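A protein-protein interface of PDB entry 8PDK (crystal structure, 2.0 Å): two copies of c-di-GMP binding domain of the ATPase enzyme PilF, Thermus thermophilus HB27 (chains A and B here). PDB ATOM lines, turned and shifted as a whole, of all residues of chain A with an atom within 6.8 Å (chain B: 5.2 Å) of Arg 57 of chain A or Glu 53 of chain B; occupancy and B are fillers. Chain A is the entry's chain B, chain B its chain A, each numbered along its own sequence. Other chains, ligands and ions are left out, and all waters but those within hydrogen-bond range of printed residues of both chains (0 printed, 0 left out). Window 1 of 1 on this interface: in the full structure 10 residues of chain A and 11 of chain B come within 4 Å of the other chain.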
ATOM      1  N   LYS A  19      29.524  -9.946 -21.296  1.00  0.00           N
ATOM      2  CA  LYS A  19      28.523 -10.968 -21.011  1.00  0.00           C
ATOM      3  C   LYS A  19      28.962 -11.885 -19.868  1.00  0.00           C
ATOM      4  O   LYS A  19      28.124 -12.361 -19.089  1.00  0.00           O
ATOM      5  CB  LYS A  19      28.241 -11.767 -22.279  1.00  0.00           C
ATOM      6  CG  LYS A  19      27.385 -11.013 -23.289  1.00  0.00           C
ATOM      7  CD  LYS A  19      27.220 -11.809 -24.561  1.00  0.00           C
ATOM      8  CE  LYS A  19      26.319 -11.093 -25.562  1.00  0.00           C
ATOM      9  NZ  LYS A  19      26.880  -9.770 -25.943  1.00  0.00           N
ATOM     10  N   TRP A  21      31.146 -14.617 -20.445  1.00  0.00           N
ATOM     11  CA  TRP A  21      31.503 -15.928 -20.975  1.00  0.00           C
ATOM     12  C   TRP A  21      32.979 -16.230 -20.818  1.00  0.00           C
ATOM     13  O   TRP A  21      33.373 -17.407 -20.821  1.00  0.00           O
ATOM     14  CB  TRP A  21      31.137 -16.008 -22.451  1.00  0.00           C
ATOM     15  CG  TRP A  21      29.698 -16.300 -22.689  1.00  0.00           C
ATOM     16  CD1 TRP A  21      28.746 -15.438 -23.157  1.00  0.00           C
ATOM     17  CD2 TRP A  21      29.045 -17.555 -22.475  1.00  0.00           C
ATOM     18  NE1 TRP A  21      27.534 -16.087 -23.245  1.00  0.00           N
ATOM     19  CE2 TRP A  21      27.693 -17.386 -22.830  1.00  0.00           C
ATOM     20  CE3 TRP A  21      29.475 -18.805 -22.015  1.00  0.00           C
ATOM     21  CZ2 TRP A  21      26.765 -18.428 -22.750  1.00  0.00           C
ATOM     22  CZ3 TRP A  21      28.548 -19.834 -21.924  1.00  0.00           C
ATOM     23  CH2 TRP A  21      27.216 -19.640 -22.302  1.00  0.00           C
ATOM     24  N   PRO A  51      30.983 -21.825 -25.799  1.00  0.00           N
ATOM     25  CA  PRO A  51      30.036 -22.490 -26.709  1.00  0.00           C
ATOM     26  C   PRO A  51      30.008 -21.790 -28.067  1.00  0.00           C
ATOM     27  O   PRO A  51      30.027 -20.561 -28.150  1.00  0.00           O
ATOM     28  CB  PRO A  51      28.686 -22.378 -25.980  1.00  0.00           C
ATOM     29  CG  PRO A  51      29.064 -22.252 -24.506  1.00  0.00           C
ATOM     30  CD  PRO A  51      30.353 -21.430 -24.528  1.00  0.00           C
ATOM     31  N   GLU A  52      29.984 -22.594 -29.139  1.00  0.00           N
ATOM     32  CA  GLU A  52      29.873 -22.033 -30.486  1.00  0.00           C
ATOM     33  C   GLU A  52      28.618 -21.181 -30.631  1.00  0.00           C
ATOM     34  O   GLU A  52      28.633 -20.146 -31.314  1.00  0.00           O
ATOM     35  CB  GLU A  52      29.882 -23.151 -31.532  1.00  0.00           C
ATOM     36  CG  GLU A  52      30.359 -22.694 -32.905  1.00  0.00           C
ATOM     37  CD  GLU A  52      30.285 -23.780 -33.977  1.00  0.00           C
ATOM     38  OE1 GLU A  52      31.157 -23.776 -34.880  1.00  0.00           O
ATOM     39  OE2 GLU A  52      29.355 -24.623 -33.929  1.00  0.00           O
ATOM     40  N   GLU A  53      27.518 -21.599 -30.003  1.00  0.00           N
ATOM     41  CA  GLU A  53      26.299 -20.813 -30.113  1.00  0.00           C
ATOM     42  C   GLU A  53      26.451 -19.464 -29.423  1.00  0.00           C
ATOM     43  O   GLU A  53      25.882 -18.470 -29.882  1.00  0.00           O
ATOM     44  CB  GLU A  53      25.097 -21.581 -29.544  1.00  0.00           C
ATOM     45  CG  GLU A  53      23.777 -20.860 -29.820  1.00  0.00           C
ATOM     46  CD  GLU A  53      22.607 -21.278 -28.917  1.00  0.00           C
ATOM     47  OE1 GLU A  53      22.845 -21.669 -27.749  1.00  0.00           O
ATOM     48  OE2 GLU A  53      21.439 -21.177 -29.380  1.00  0.00           O
ATOM     49  N   ALA A  54      27.218 -19.402 -28.328  1.00  0.00           N
ATOM     50  CA  ALA A  54      27.457 -18.113 -27.688  1.00  0.00           C
ATOM     51  C   ALA A  54      28.350 -17.230 -28.548  1.00  0.00           C
ATOM     52  O   ALA A  54      28.166 -16.003 -28.602  1.00  0.00           O
ATOM     53  CB  ALA A  54      28.078 -18.310 -26.309  1.00  0.00           C
ATOM     54  N   LEU A  55      29.343 -17.822 -29.204  1.00  0.00           N
ATOM     55  CA  LEU A  55      30.177 -17.030 -30.102  1.00  0.00           C
ATOM     56  C   LEU A  55      29.328 -16.392 -31.193  1.00  0.00           C
ATOM     57  O   LEU A  55      29.447 -15.197 -31.476  1.00  0.00           O
ATOM     58  CB  LEU A  55      31.263 -17.903 -30.725  1.00  0.00           C
ATOM     59  CG  LEU A  55      32.009 -17.220 -31.869  1.00  0.00           C
ATOM     60  CD1 LEU A  55      32.753 -15.994 -31.347  1.00  0.00           C
ATOM     61  CD2 LEU A  55      32.974 -18.232 -32.492  1.00  0.00           C
ATOM     62  N   TYR A  56      28.439 -17.181 -31.792  1.00  0.00           N
ATOM     63  CA  TYR A  56      27.681 -16.700 -32.942  1.00  0.00           C
ATOM     64  C   TYR A  56      26.651 -15.657 -32.541  1.00  0.00           C
ATOM     65  O   TYR A  56      26.355 -14.744 -33.322  1.00  0.00           O
ATOM     66  CB  TYR A  56      27.034 -17.896 -33.646  1.00  0.00           C
ATOM     67  CG  TYR A  56      27.927 -18.427 -34.733  1.00  0.00           C
ATOM     68  CD1 TYR A  56      29.259 -18.734 -34.469  1.00  0.00           C
ATOM     69  CD2 TYR A  56      27.464 -18.563 -36.040  1.00  0.00           C
ATOM     70  CE1 TYR A  56      30.099 -19.191 -35.470  1.00  0.00           C
ATOM     71  CE2 TYR A  56      28.294 -19.026 -37.045  1.00  0.00           C
ATOM     72  CZ  TYR A  56      29.613 -19.332 -36.757  1.00  0.00           C
ATOM     73  OH  TYR A  56      30.443 -19.790 -37.757  1.00  0.00           O
ATOM     74  N   ARG A  57      26.100 -15.762 -31.328  1.00  0.00           N
ATOM     75  CA  ARG A  57      25.178 -14.728 -30.869  1.00  0.00           C
ATOM     76  C   ARG A  57      25.898 -13.394 -30.710  1.00  0.00           C
ATOM     77  O   ARG A  57      25.380 -12.347 -31.125  1.00  0.00           O
ATOM     78  CB  ARG A  57      24.501 -15.149 -29.553  1.00  0.00           C
ATOM     79  CG  ARG A  57      23.344 -16.139 -29.730  1.00  0.00           C
ATOM     80  CD  ARG A  57      22.440 -16.220 -28.479  1.00  0.00           C
ATOM     81  NE  ARG A  57      23.227 -16.508 -27.289  1.00  0.00           N
ATOM     82  CZ  ARG A  57      23.444 -17.733 -26.818  1.00  0.00           C
ATOM     83  NH1 ARG A  57      22.909 -18.778 -27.430  1.00  0.00           N
ATOM     84  NH2 ARG A  57      24.183 -17.913 -25.728  1.00  0.00           N
ATOM     85  N   ALA A  58      27.101 -13.413 -30.136  1.00  0.00           N
ATOM     86  CA  ALA A  58      27.896 -12.186 -30.027  1.00  0.00           C
ATOM     87  C   ALA A  58      28.278 -11.621 -31.404  1.00  0.00           C
ATOM     88  O   ALA A  58      28.210 -10.404 -31.621  1.00  0.00           O
ATOM     89  CB  ALA A  58      29.154 -12.455 -29.201  1.00  0.00           C
ATOM     90  N   LEU A  59      28.710 -12.482 -32.333  1.00  0.00           N
ATOM     91  CA  LEU A  59      29.087 -12.001 -33.667  1.00  0.00           C
ATOM     92  C   LEU A  59      27.883 -11.421 -34.395  1.00  0.00           C
ATOM     93  O   LEU A  59      28.007 -10.444 -35.142  1.00  0.00           O
ATOM     94  CB  LEU A  59      29.702 -13.138 -34.488  1.00  0.00           C
ATOM     95  CG  LEU A  59      31.100 -13.639 -34.104  1.00  0.00           C
ATOM     96  CD1 LEU A  59      31.431 -14.978 -34.762  1.00  0.00           C
ATOM     97  CD2 LEU A  59      32.170 -12.603 -34.451  1.00  0.00           C
ATOM     98  N   ALA A  60      26.707 -12.025 -34.183  1.00  0.00           N
ATOM     99  CA  ALA A  60      25.460 -11.517 -34.742  1.00  0.00           C
ATOM    100  C   ALA A  60      25.111 -10.146 -34.173  1.00  0.00           C
ATOM    101  O   ALA A  60      24.715  -9.241 -34.915  1.00  0.00           O
ATOM    102  CB  ALA A  60      24.329 -12.517 -34.475  1.00  0.00           C
ATOM    103  N   GLU A  61      25.235  -9.977 -32.849  1.00  0.00           N
ATOM    104  CA  GLU A  61      24.989  -8.669 -32.236  1.00  0.00           C
ATOM    105  C   GLU A  61      25.951  -7.614 -32.763  1.00  0.00           C
ATOM    106  O   GLU A  61      25.564  -6.455 -32.972  1.00  0.00           O
ATOM    107  CB  GLU A  61      25.131  -8.756 -30.723  1.00  0.00           C
ATOM    108  CG  GLU A  61      23.952  -9.340 -30.016  1.00  0.00           C
ATOM    109  CD  GLU A  61      24.205  -9.438 -28.529  1.00  0.00           C
ATOM    110  OE1 GLU A  61      24.733  -8.453 -27.955  1.00  0.00           O
ATOM    111  OE2 GLU A  61      23.899 -10.501 -27.948  1.00  0.00           O
ATOM    112  N   GLN A  62      27.218  -7.993 -32.957  1.00  0.00           N
ATOM    113  CA  GLN A  62      28.234  -7.034 -33.390  1.00  0.00           C
ATOM    114  C   GLN A  62      27.940  -6.492 -34.788  1.00  0.00           C
ATOM    115  O   GLN A  62      28.258  -5.335 -35.084  1.00  0.00           O
ATOM    116  CB  GLN A  62      29.614  -7.699 -33.326  1.00  0.00           C
ATOM    117  CG  GLN A  62      30.772  -6.921 -33.935  1.00  0.00           C
ATOM    118  CD  GLN A  62      32.056  -7.748 -33.956  1.00  0.00           C
ATOM    119  OE1 GLN A  62      32.186  -8.680 -34.738  1.00  0.00           O
ATOM    120  NE2 GLN A  62      32.996  -7.419 -33.079  1.00  0.00           N
ATOM    121  N   LEU A  65      23.030  -8.673 -37.028  1.00  0.00           N
ATOM    122  CA  LEU A  65      22.366  -9.840 -37.574  1.00  0.00           C
ATOM    123  C   LEU A  65      21.447 -10.433 -36.530  1.00  0.00           C
ATOM    124  O   LEU A  65      21.634 -10.240 -35.327  1.00  0.00           O
ATOM    125  CB  LEU A  65      23.382 -10.896 -38.009  1.00  0.00           C
ATOM    126  CG  LEU A  65      24.325 -10.480 -39.128  1.00  0.00           C
ATOM    127  CD1 LEU A  65      25.726 -10.871 -38.803  1.00  0.00           C
ATOM    128  CD2 LEU A  65      23.861 -11.211 -40.343  1.00  0.00           C
ATOM    129  N   PHE A  67      20.605 -13.884 -34.948  1.00  0.00           N
ATOM    130  CA  PHE A  67      21.037 -15.267 -34.866  1.00  0.00           C
ATOM    131  C   PHE A  67      19.823 -16.187 -34.850  1.00  0.00           C
ATOM    132  O   PHE A  67      18.836 -15.916 -34.169  1.00  0.00           O
ATOM    133  CB  PHE A  67      21.894 -15.516 -33.624  1.00  0.00           C
ATOM    134  CG  PHE A  67      22.337 -16.943 -33.498  1.00  0.00           C
ATOM    135  CD1 PHE A  67      23.210 -17.487 -34.423  1.00  0.00           C
ATOM    136  CD2 PHE A  67      21.852 -17.754 -32.489  1.00  0.00           C
ATOM    137  CE1 PHE A  67      23.616 -18.802 -34.340  1.00  0.00           C
ATOM    138  CE2 PHE A  67      22.253 -19.076 -32.397  1.00  0.00           C
ATOM    139  CZ  PHE A  67      23.138 -19.599 -33.318  1.00  0.00           C
ATOM    140  N   GLU A  69      18.672 -19.835 -33.871  1.00  0.00           N
ATOM    141  CA  GLU A  69      19.077 -21.043 -33.158  1.00  0.00           C
ATOM    142  C   GLU A  69      18.797 -22.302 -33.966  1.00  0.00           C
ATOM    143  O   GLU A  69      19.404 -23.346 -33.703  1.00  0.00           O
ATOM    144  CB  GLU A  69      18.370 -21.125 -31.809  1.00  0.00           C
ATOM    145  CG  GLU A  69      18.235 -19.803 -31.103  1.00  0.00           C
ATOM    146  CD  GLU A  69      16.995 -19.751 -30.222  1.00  0.00           C
ATOM    147  OE1 GLU A  69      16.165 -20.692 -30.295  1.00  0.00           O
ATOM    148  OE2 GLU A  69      16.865 -18.779 -29.440  1.00  0.00           O
ATOM    149  N   LEU A 129      21.909 -15.044 -39.134  1.00  0.00           N
ATOM    150  CA  LEU A 129      23.134 -15.822 -39.010  1.00  0.00           C
ATOM    151  C   LEU A 129      22.792 -17.189 -38.441  1.00  0.00           C
ATOM    152  O   LEU A 129      21.993 -17.297 -37.504  1.00  0.00           O
ATOM    153  CB  LEU A 129      24.181 -15.112 -38.106  1.00  0.00           C
ATOM    154  CG  LEU A 129      25.491 -15.885 -37.906  1.00  0.00           C
ATOM    155  CD1 LEU A 129      26.340 -15.939 -39.202  1.00  0.00           C
ATOM    156  CD2 LEU A 129      26.305 -15.294 -36.750  1.00  0.00           C
ATOM    157  N   PRO B  51      25.940 -15.765 -17.509  1.00  0.00           N
ATOM    158  CA  PRO B  51      24.886 -15.972 -18.514  1.00  0.00           C
ATOM    159  C   PRO B  51      24.021 -17.142 -18.089  1.00  0.00           C
ATOM    160  O   PRO B  51      24.524 -18.179 -17.653  1.00  0.00           O
ATOM    161  CB  PRO B  51      25.649 -16.269 -19.813  1.00  0.00           C
ATOM    162  CG  PRO B  51      27.044 -15.670 -19.588  1.00  0.00           C
ATOM    163  CD  PRO B  51      27.295 -15.803 -18.085  1.00  0.00           C
ATOM    164  N   GLU B  52      22.709 -16.955 -18.194  1.00  0.00           N
ATOM    165  CA  GLU B  52      21.779 -18.015 -17.823  1.00  0.00           C
ATOM    166  C   GLU B  52      22.055 -19.303 -18.600  1.00  0.00           C
ATOM    167  O   GLU B  52      21.900 -20.408 -18.064  1.00  0.00           O
ATOM    168  CB  GLU B  52      20.358 -17.506 -18.048  1.00  0.00           C
ATOM    169  CG  GLU B  52      19.272 -18.528 -18.006  1.00  0.00           C
ATOM    170  CD  GLU B  52      17.967 -17.937 -18.494  1.00  0.00           C
ATOM    171  OE1 GLU B  52      17.832 -17.721 -19.726  1.00  0.00           O
ATOM    172  OE2 GLU B  52      17.096 -17.664 -17.643  1.00  0.00           O
ATOM    173  N   GLU B  53      22.504 -19.185 -19.848  1.00  0.00           N
ATOM    174  CA  GLU B  53      22.800 -20.385 -20.610  1.00  0.00           C
ATOM    175  C   GLU B  53      24.040 -21.088 -20.088  1.00  0.00           C
ATOM    176  O   GLU B  53      24.142 -22.321 -20.175  1.00  0.00           O
ATOM    177  CB  GLU B  53      22.972 -20.040 -22.085  1.00  0.00           C
ATOM    178  CG  GLU B  53      23.031 -21.260 -22.953  1.00  0.00           C
ATOM    179  CD  GLU B  53      23.216 -20.913 -24.410  1.00  0.00           C
ATOM    180  OE1 GLU B  53      22.194 -20.621 -25.076  1.00  0.00           O
ATOM    181  OE2 GLU B  53      24.382 -20.932 -24.870  1.00  0.00           O
ATOM    182  N   ALA B  54      25.006 -20.329 -19.570  1.00  0.00           N
ATOM    183  CA  ALA B  54      26.157 -20.973 -18.946  1.00  0.00           C
ATOM    184  C   ALA B  54      25.714 -21.772 -17.727  1.00  0.00           C
ATOM    185  O   ALA B  54      26.187 -22.890 -17.496  1.00  0.00           O
ATOM    186  CB  ALA B  54      27.221 -19.925 -18.574  1.00  0.00           C
ATOM    187  N   LEU B  55      24.798 -21.208 -16.939  1.00  0.00           N
ATOM    188  CA  LEU B  55      24.198 -21.946 -15.831  1.00  0.00           C
ATOM    189  C   LEU B  55      23.536 -23.227 -16.325  1.00  0.00           C
ATOM    190  O   LEU B  55      23.768 -24.310 -15.778  1.00  0.00           O
ATOM    191  CB  LEU B  55      23.177 -21.057 -15.102  1.00  0.00           C
ATOM    192  CG  LEU B  55      22.352 -21.737 -13.988  1.00  0.00           C
ATOM    193  CD1 LEU B  55      23.256 -22.291 -12.913  1.00  0.00           C
ATOM    194  CD2 LEU B  55      21.366 -20.767 -13.391  1.00  0.00           C
ATOM    195  N   TYR B  56      22.724 -23.131 -17.383  1.00  0.00           N
ATOM    196  CA  TYR B  56      21.943 -24.295 -17.798  1.00  0.00           C
ATOM    197  C   TYR B  56      22.819 -25.383 -18.410  1.00  0.00           C
ATOM    198  O   TYR B  56      22.594 -26.578 -18.169  1.00  0.00           O
ATOM    199  CB  TYR B  56      20.828 -23.857 -18.752  1.00  0.00           C
ATOM    200  CG  TYR B  56      19.587 -23.535 -17.956  1.00  0.00           C
ATOM    201  CD1 TYR B  56      19.540 -22.396 -17.153  1.00  0.00           C
ATOM    202  CD2 TYR B  56      18.484 -24.377 -17.970  1.00  0.00           C
ATOM    203  CE1 TYR B  56      18.427 -22.100 -16.392  1.00  0.00           C
ATOM    204  CE2 TYR B  56      17.354 -24.086 -17.203  1.00  0.00           C
ATOM    205  CZ  TYR B  56      17.339 -22.952 -16.413  1.00  0.00           C
ATOM    206  OH  TYR B  56      16.236 -22.646 -15.649  1.00  0.00           O
ATOM    207  N   ARG B  57      23.840 -24.994 -19.165  1.00  0.00           N
ATOM    208  CA  ARG B  57      24.787 -25.966 -19.709  1.00  0.00           C
ATOM    209  C   ARG B  57      25.500 -26.734 -18.600  1.00  0.00           C
ATOM    210  O   ARG B  57      25.640 -27.959 -18.667  1.00  0.00           O
ATOM    211  CB  ARG B  57      25.810 -25.246 -20.593  1.00  0.00           C
ATOM    212  CG  ARG B  57      25.250 -24.826 -21.946  1.00  0.00           C
ATOM    213  CD  ARG B  57      26.344 -24.129 -22.778  1.00  0.00           C
ATOM    214  NE  ARG B  57      25.755 -23.570 -24.006  1.00  0.00           N
ATOM    215  CZ  ARG B  57      25.583 -24.268 -25.124  1.00  0.00           C
ATOM    216  NH1 ARG B  57      25.028 -23.700 -26.192  1.00  0.00           N
ATOM    217  NH2 ARG B  57      25.975 -25.538 -25.169  1.00  0.00           N
ATOM    218  N   ALA B  58      25.974 -26.022 -17.573  1.00  0.00           N
ATOM    219  CA  ALA B  58      26.624 -26.705 -16.456  1.00  0.00           C
ATOM    220  C   ALA B  58      25.637 -27.599 -15.706  1.00  0.00           C
ATOM    221  O   ALA B  58      25.962 -28.743 -15.368  1.00  0.00           O
ATOM    222  CB  ALA B  58      27.253 -25.688 -15.506  1.00  0.00           C
ATOM    223  N   PHE B  67      21.720 -30.593 -23.165  1.00  0.00           N
ATOM    224  CA  PHE B  67      21.208 -29.236 -23.226  1.00  0.00           C
ATOM    225  C   PHE B  67      20.726 -28.947 -24.643  1.00  0.00           C
ATOM    226  O   PHE B  67      21.416 -29.259 -25.614  1.00  0.00           O
ATOM    227  CB  PHE B  67      22.281 -28.222 -22.808  1.00  0.00           C
ATOM    228  CG  PHE B  67      21.836 -26.797 -22.966  1.00  0.00           C
ATOM    229  CD1 PHE B  67      20.828 -26.288 -22.171  1.00  0.00           C
ATOM    230  CD2 PHE B  67      22.381 -25.985 -23.958  1.00  0.00           C
ATOM    231  CE1 PHE B  67      20.381 -24.986 -22.320  1.00  0.00           C
ATOM    232  CE2 PHE B  67      21.941 -24.665 -24.115  1.00  0.00           C
ATOM    233  CZ  PHE B  67      20.943 -24.170 -23.296  1.00  0.00           C
ATOM    234  N   LEU B 131      16.146 -23.953 -21.856  1.00  0.00           N
ATOM    235  CA  LEU B 131      15.981 -22.674 -21.187  1.00  0.00           C
ATOM    236  C   LEU B 131      14.497 -22.374 -20.977  1.00  0.00           C
ATOM    237  O   LEU B 131      13.640 -22.884 -21.708  1.00  0.00           O
ATOM    238  CB  LEU B 131      16.639 -21.555 -22.016  1.00  0.00           C
ATOM    239  CG  LEU B 131      18.166 -21.655 -22.115  1.00  0.00           C
ATOM    240  CD1 LEU B 131      18.769 -20.857 -23.310  1.00  0.00           C
ATOM    241  CD2 LEU B 131      18.767 -21.229 -20.797  1.00  0.00           C
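The guanidinium group (NH1) of Arg 57 of chain A is in salt-bridge range of the side-chain carboxylate (OE1) of Glu 53 of chain B (3.1 Å).
NH1 of Arg 57 of chain B lies within salt-bridge range of OE1 of Glu 53 of chain A, 3.4 Å away.
OE1 of Glu 53 of chain A sits close to OE1 of Glu 53 of chain B (2.9 Å).
The side-chain carboxylate (OE2) of Glu 53 of chain B lies within salt-bridge range of the guanidinium group (NE) of Arg 57 of chain B (3.1 Å).
The side-chain amino group (NZ) of Lys 19 of chain A lies within salt-bridge range of the side-chain carboxylate (OE1) of Glu 61 of chain A, 3.2 Å away.
The side-chain carboxylate of Glu 53 of chain A is in salt-bridge range of the guanidinium group of Arg 57 of chain A (2.9 Å).
Among the printed residues, merely in contact across the chains: Lys 19 of chain A with Pro 51 of chain B, Trp 21 of chain A with Pro 51 of chain B, Trp 21 of chain A with Ala 54 of chain B and Pro 51 of chain A with Arg 57 of chain B.
Of chain A, only Glu 53 (2.9 Å) and Arg 57 (3.1 Å) come within 4 Å of Glu 53 of chain B.
Printed residues of chain A within 4 Å of Pro 51 of chain B: Lys 19 (3.5 Å) and Trp 21 (3.7 Å).
Of the printed residues of chain B, Lys 19 of chain A touches Pro 51.
Tyr 56 of chain B touches none of the printed residues of chain A.
The nearest printed residue of chain B that does not touch Arg 57 of chain A is Arg 57 of chain B (5.5 Å).
The nearest printed residue of chain A that does not touch Arg 57 of chain B is Trp 21 of chain A (4.5 Å).
Of the 18 printed residues of chain A, 5 touch a printed residue of chain B.
Printed residues of chain A that touch a printed residue of chain B: Lys 19, Trp 21, Pro 51, Glu 53 and Arg 57.
Hydrophobic or aromatic side chains of chain B that line the printed part of chain A: Pro 51 and Ala 54.
Among the printed residues, Asp or Glu carboxylates within 4 Å of a Lys or Arg side-chain nitrogen of the other chain: Glu 53 of chain A with Arg 57 of chain B and Arg 57 of chain A with Glu 53 of chain B.
Pro 51 of chain A touches Arg 57 of chain B, but with the chains exchanged Arg 57 of chain A does not touch Pro 51 of chain B (6.3 Å).
Glu 53 of chain A touches its own counterpart, Glu 53 of chain B.
Glu 53 of chain A touches Arg 57 of chain B, and with the chains exchanged Arg 57 of chain A touches Glu 53 of chain B.
Of the 7 pairs that touch across the chains among the printed residues, 3 have their exchanged pair printed and touching as well.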
